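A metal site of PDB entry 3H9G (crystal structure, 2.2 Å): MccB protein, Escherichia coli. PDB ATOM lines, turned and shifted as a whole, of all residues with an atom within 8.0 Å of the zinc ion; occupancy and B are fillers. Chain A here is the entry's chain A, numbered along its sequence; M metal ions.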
ATOM      1  N   ASN A 227     -16.908   3.392 -26.198  1.00  0.00           N
ATOM      2  CA  ASN A 227     -18.122   3.966 -25.635  1.00  0.00           C
ATOM      3  C   ASN A 227     -17.842   4.731 -24.355  1.00  0.00           C
ATOM      4  O   ASN A 227     -18.139   5.930 -24.281  1.00  0.00           O
ATOM      5  CB  ASN A 227     -19.184   2.888 -25.395  1.00  0.00           C
ATOM      6  CG  ASN A 227     -20.462   3.462 -24.839  1.00  0.00           C
ATOM      7  OD1 ASN A 227     -21.125   4.280 -25.479  1.00  0.00           O
ATOM      8  ND2 ASN A 227     -20.798   3.071 -23.615  1.00  0.00           N
ATOM      9  N   VAL A 231     -18.253   8.684 -24.056  1.00  0.00           N
ATOM     10  CA  VAL A 231     -19.205   9.290 -23.125  1.00  0.00           C
ATOM     11  C   VAL A 231     -18.489  10.356 -22.289  1.00  0.00           C
ATOM     12  O   VAL A 231     -18.962  11.479 -22.171  1.00  0.00           O
ATOM     13  CB  VAL A 231     -19.912   8.250 -22.217  1.00  0.00           C
ATOM     14  CG1 VAL A 231     -20.691   8.949 -21.103  1.00  0.00           C
ATOM     15  CG2 VAL A 231     -20.841   7.344 -23.029  1.00  0.00           C
ATOM     16  N   TYR A 253     -23.810   7.270 -31.357  1.00  0.00           N
ATOM     17  CA  TYR A 253     -23.864   7.940 -30.065  1.00  0.00           C
ATOM     18  C   TYR A 253     -23.668   9.452 -30.188  1.00  0.00           C
ATOM     19  O   TYR A 253     -22.685   9.921 -30.743  1.00  0.00           O
ATOM     20  CB  TYR A 253     -22.863   7.332 -29.082  1.00  0.00           C
ATOM     21  CG  TYR A 253     -22.676   8.107 -27.797  1.00  0.00           C
ATOM     22  CD1 TYR A 253     -23.642   8.068 -26.804  1.00  0.00           C
ATOM     23  CD2 TYR A 253     -21.542   8.881 -27.581  1.00  0.00           C
ATOM     24  CE1 TYR A 253     -23.496   8.769 -25.638  1.00  0.00           C
ATOM     25  CE2 TYR A 253     -21.373   9.603 -26.394  1.00  0.00           C
ATOM     26  CZ  TYR A 253     -22.369   9.529 -25.438  1.00  0.00           C
ATOM     27  OH  TYR A 253     -22.265  10.215 -24.250  1.00  0.00           O
ATOM     28  N   THR A 258     -28.752  10.838 -26.934  1.00  0.00           N
ATOM     29  CA  THR A 258     -28.937   9.459 -27.326  1.00  0.00           C
ATOM     30  C   THR A 258     -28.439   8.499 -26.229  1.00  0.00           C
ATOM     31  O   THR A 258     -27.703   8.906 -25.336  1.00  0.00           O
ATOM     32  CB  THR A 258     -28.247   9.208 -28.698  1.00  0.00           C
ATOM     33  OG1 THR A 258     -29.011   8.297 -29.495  1.00  0.00           O
ATOM     34  CG2 THR A 258     -26.835   8.670 -28.522  1.00  0.00           C
ATOM     35  N   GLY A 259     -28.871   7.241 -26.283  1.00  0.00           N
ATOM     36  CA  GLY A 259     -28.347   6.224 -25.383  1.00  0.00           C
ATOM     37  C   GLY A 259     -26.931   5.851 -25.766  1.00  0.00           C
ATOM     38  O   GLY A 259     -26.518   6.074 -26.909  1.00  0.00           O
ATOM     39  N   CYS A 260     -26.173   5.320 -24.809  1.00  0.00           N
ATOM     40  CA  CYS A 260     -24.839   4.802 -25.092  1.00  0.00           C
ATOM     41  C   CYS A 260     -24.921   3.299 -25.315  1.00  0.00           C
ATOM     42  O   CYS A 260     -25.995   2.702 -25.181  1.00  0.00           O
ATOM     43  CB  CYS A 260     -23.839   5.165 -23.982  1.00  0.00           C
ATOM     44  SG  CYS A 260     -23.771   4.040 -22.546  1.00  0.00           S
ATOM     45  N   TYR A 261     -23.788   2.698 -25.674  1.00  0.00           N
ATOM     46  CA  TYR A 261     -23.707   1.269 -25.959  1.00  0.00           C
ATOM     47  C   TYR A 261     -24.193   0.434 -24.762  1.00  0.00           C
ATOM     48  O   TYR A 261     -24.870  -0.573 -24.935  1.00  0.00           O
ATOM     49  CB  TYR A 261     -22.278   0.894 -26.340  1.00  0.00           C
ATOM     50  CG  TYR A 261     -22.129  -0.425 -27.058  1.00  0.00           C
ATOM     51  CD1 TYR A 261     -22.491  -0.553 -28.403  1.00  0.00           C
ATOM     52  CD2 TYR A 261     -21.623  -1.540 -26.401  1.00  0.00           C
ATOM     53  CE1 TYR A 261     -22.364  -1.759 -29.071  1.00  0.00           C
ATOM     54  CE2 TYR A 261     -21.478  -2.761 -27.064  1.00  0.00           C
ATOM     55  CZ  TYR A 261     -21.858  -2.861 -28.393  1.00  0.00           C
ATOM     56  OH  TYR A 261     -21.708  -4.059 -29.060  1.00  0.00           O
ATOM     57  N   GLU A 262     -23.866   0.897 -23.560  1.00  0.00           N
ATOM     58  CA  GLU A 262     -24.178   0.156 -22.328  1.00  0.00           C
ATOM     59  C   GLU A 262     -25.621   0.281 -21.805  1.00  0.00           C
ATOM     60  O   GLU A 262     -26.052  -0.586 -21.041  1.00  0.00           O
ATOM     61  CB  GLU A 262     -23.199   0.530 -21.210  1.00  0.00           C
ATOM     62  CG  GLU A 262     -22.225  -0.584 -20.834  1.00  0.00           C
ATOM     63  CD  GLU A 262     -21.378  -1.052 -21.991  1.00  0.00           C
ATOM     64  OE1 GLU A 262     -20.531  -0.269 -22.494  1.00  0.00           O
ATOM     65  OE2 GLU A 262     -21.551  -2.231 -22.390  1.00  0.00           O
ATOM     66  N   CYS A 263     -26.341   1.322 -22.215  1.00  0.00           N
ATOM     67  CA  CYS A 263     -27.671   1.618 -21.639  1.00  0.00           C
ATOM     68  C   CYS A 263     -28.626   0.428 -21.524  1.00  0.00           C
ATOM     69  O   CYS A 263     -29.127   0.114 -20.448  1.00  0.00           O
ATOM     70  CB  CYS A 263     -28.338   2.764 -22.393  1.00  0.00           C
ATOM     71  SG  CYS A 263     -27.753   4.375 -21.893  1.00  0.00           S
ATOM     72  N   GLN A 264     -28.874  -0.234 -22.650  1.00  0.00           N
ATOM     73  CA  GLN A 264     -29.898  -1.269 -22.737  1.00  0.00           C
ATOM     74  C   GLN A 264     -29.374  -2.688 -22.487  1.00  0.00           C
ATOM     75  O   GLN A 264     -30.164  -3.606 -22.288  1.00  0.00           O
ATOM     76  CB  GLN A 264     -30.634  -1.186 -24.075  1.00  0.00           C
ATOM     77  CG  GLN A 264     -31.434   0.080 -24.251  1.00  0.00           C
ATOM     78  CD  GLN A 264     -32.265   0.425 -23.024  1.00  0.00           C
ATOM     79  OE1 GLN A 264     -32.986  -0.423 -22.487  1.00  0.00           O
ATOM     80  NE2 GLN A 264     -32.163   1.665 -22.569  1.00  0.00           N
ATOM     81  N   LYS A 265     -28.053  -2.834 -22.490  1.00  0.00           N
ATOM     82  CA  LYS A 265     -27.400  -4.138 -22.310  1.00  0.00           C
ATOM     83  C   LYS A 265     -27.999  -5.179 -23.257  1.00  0.00           C
ATOM     84  O   LYS A 265     -28.653  -6.137 -22.813  1.00  0.00           O
ATOM     85  CB  LYS A 265     -27.482  -4.598 -20.834  1.00  0.00           C
ATOM     86  N   MET A 340     -31.360   0.938 -28.330  1.00  0.00           N
ATOM     87  CA  MET A 340     -30.201   1.427 -27.616  1.00  0.00           C
ATOM     88  C   MET A 340     -30.438   2.858 -27.122  1.00  0.00           C
ATOM     89  O   MET A 340     -29.528   3.690 -27.117  1.00  0.00           O
ATOM     90  CB  MET A 340     -28.944   1.338 -28.482  1.00  0.00           C
ATOM     91  CG  MET A 340     -28.498  -0.077 -28.754  1.00  0.00           C
ATOM     92  SD  MET A 340     -26.718  -0.222 -28.936  1.00  0.00           S
ATOM     93  CE  MET A 340     -26.558  -1.982 -28.612  1.00  0.00           C
ATOM     94  N   GLY A 341     -31.666   3.129 -26.714  1.00  0.00           N
ATOM     95  CA  GLY A 341     -32.037   4.422 -26.146  1.00  0.00           C
ATOM     96  C   GLY A 341     -31.486   4.597 -24.736  1.00  0.00           C
ATOM     97  O   GLY A 341     -31.056   3.626 -24.108  1.00  0.00           O
ATOM     98  N   ARG A 342     -31.523   5.825 -24.241  1.00  0.00           N
ATOM     99  CA  ARG A 342     -30.929   6.140 -22.935  1.00  0.00           C
ATOM    100  C   ARG A 342     -31.608   5.402 -21.775  1.00  0.00           C
ATOM    101  O   ARG A 342     -32.815   5.162 -21.782  1.00  0.00           O
ATOM    102  CB  ARG A 342     -30.922   7.658 -22.676  1.00  0.00           C
ATOM    103  CG  ARG A 342     -29.824   8.107 -21.710  1.00  0.00           C
ATOM    104  CD  ARG A 342     -29.968   9.568 -21.308  1.00  0.00           C
ATOM    105  NE  ARG A 342     -31.070   9.765 -20.358  1.00  0.00           N
ATOM    106  CZ  ARG A 342     -30.933   9.913 -19.043  1.00  0.00           C
ATOM    107  NH1 ARG A 342     -29.726   9.899 -18.475  1.00  0.00           N
ATOM    108  NH2 ARG A 342     -32.011  10.075 -18.291  1.00  0.00           N
ATOM    109  N   SER A 343     -30.789   5.009 -20.800  1.00  0.00           N
ATOM    110  CA  SER A 343     -31.272   4.488 -19.540  1.00  0.00           C
ATOM    111  C   SER A 343     -30.787   5.367 -18.398  1.00  0.00           C
ATOM    112  O   SER A 343     -29.572   5.577 -18.253  1.00  0.00           O
ATOM    113  CB  SER A 343     -30.793   3.050 -19.309  1.00  0.00           C
ATOM    114  OG  SER A 343     -31.091   2.625 -17.996  1.00  0.00           O
ATOM    115  N   PRO A 344     -31.728   5.902 -17.581  1.00  0.00           N
ATOM    116  CA  PRO A 344     -31.354   6.739 -16.437  1.00  0.00           C
ATOM    117  C   PRO A 344     -30.481   5.960 -15.455  1.00  0.00           C
ATOM    118  O   PRO A 344     -29.639   6.543 -14.785  1.00  0.00           O
ATOM    119  CB  PRO A 344     -32.712   7.060 -15.787  1.00  0.00           C
ATOM    120  CG  PRO A 344     -33.711   6.872 -16.870  1.00  0.00           C
ATOM    121  CD  PRO A 344     -33.194   5.743 -17.695  1.00  0.00           C
ATOM    122  N   VAL A 345     -30.689   4.640 -15.435  1.00  0.00           N
ATOM    123  CA  VAL A 345     -30.000   3.700 -14.557  1.00  0.00           C
ATOM    124  C   VAL A 345     -28.560   3.392 -15.016  1.00  0.00           C
ATOM    125  O   VAL A 345     -27.736   2.916 -14.225  1.00  0.00           O
ATOM    126  CB  VAL A 345     -30.823   2.378 -14.434  1.00  0.00           C
ATOM    127  CG1 VAL A 345     -30.113   1.373 -13.540  1.00  0.00           C
ATOM    128  CG2 VAL A 345     -32.210   2.667 -13.875  1.00  0.00           C
ATOM    129  N   CYS A 346     -28.251   3.659 -16.276  1.00  0.00           N
ATOM    130  CA  CYS A 346     -26.946   3.318 -16.845  1.00  0.00           C
ATOM    131  C   CYS A 346     -25.799   3.772 -15.952  1.00  0.00           C
ATOM    132  O   CYS A 346     -25.809   4.891 -15.441  1.00  0.00           O
ATOM    133  CB  CYS A 346     -26.791   3.903 -18.251  1.00  0.00           C
ATOM    134  SG  CYS A 346     -25.333   3.325 -19.166  1.00  0.00           S
ATOM    135  N   SER A 347     -24.821   2.904 -15.753  1.00  0.00           N
ATOM    136  CA  SER A 347     -23.680   3.196 -14.890  1.00  0.00           C
ATOM    137  C   SER A 347     -22.556   3.877 -15.660  1.00  0.00           C
ATOM    138  O   SER A 347     -21.536   4.247 -15.084  1.00  0.00           O
ATOM    139  CB  SER A 347     -23.164   1.919 -14.221  1.00  0.00           C
ATOM    140  OG  SER A 347     -22.741   0.976 -15.186  1.00  0.00           O
ATOM    141  N   VAL A 348     -22.757   4.039 -16.961  1.00  0.00           N
ATOM    142  CA  VAL A 348     -21.750   4.644 -17.823  1.00  0.00           C
ATOM    143  C   VAL A 348     -22.087   6.105 -18.144  1.00  0.00           C
ATOM    144  O   VAL A 348     -21.217   6.970 -18.079  1.00  0.00           O
ATOM    145  CB  VAL A 348     -21.537   3.820 -19.111  1.00  0.00           C
ATOM    146  CG1 VAL A 348     -20.402   4.387 -19.951  1.00  0.00           C
ATOM    147  CG2 VAL A 348     -21.240   2.371 -18.756  1.00  0.00           C
ATOM    148  N   CYS A 349     -23.343   6.362 -18.503  1.00  0.00           N
ATOM    149  CA  CYS A 349     -23.753   7.711 -18.873  1.00  0.00           C
ATOM    150  C   CYS A 349     -24.890   8.258 -18.003  1.00  0.00           C
ATOM    151  O   CYS A 349     -25.347   9.377 -18.222  1.00  0.00           O
ATOM    152  CB  CYS A 349     -24.139   7.751 -20.364  1.00  0.00           C
ATOM    153  SG  CYS A 349     -25.662   6.878 -20.786  1.00  0.00           S
ATOM    154  N   GLY A 350     -25.338   7.458 -17.042  1.00  0.00           N
ATOM    155  CA  GLY A 350     -26.481   7.806 -16.195  1.00  0.00           C
ATOM    156  C   GLY A 350     -26.120   8.464 -14.870  1.00  0.00           C
ATOM    157  O   GLY A 350     -24.998   8.953 -14.707  1.00  0.00           O
HETATM  158 ZN    ZN M   1     -25.576   4.623 -21.177  1.00  0.00          ZN
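The side-chain sulfur of Cys 263 lies close to the backbone NH of Ser 343, at 3.3 Å.
SG of Cys 260 sits close to N of Glu 262, 3.3 Å away.
The side-chain sulfur of Cys 260 sits close to the side-chain amide nitrogen of Asn 227 (3.3 Å).
The side-chain sulfur of Cys 346 sits close to the backbone NH of Val 348 (3.5 Å).
The side-chain hydroxyl (OG) of Ser 343 lies within hydrogen-bond range of the backbone NH (N) of Cys 346 (3.5 Å).
Within 4 Å of the zinc ion: Cys 260, Cys 263, Cys 346 and Cys 349.
The nearest printed residue that does not touch the zinc ion is Glu 262 (4.4 Å).
The zinc ion is bound by the side-chain sulfur of Cys 349 (2.3 Å), the side-chain sulfur of Cys 263 (2.3 Å), the side-chain sulfur of Cys 260 (2.3 Å) and the side-chain sulfur of Cys 346 (2.4 Å).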
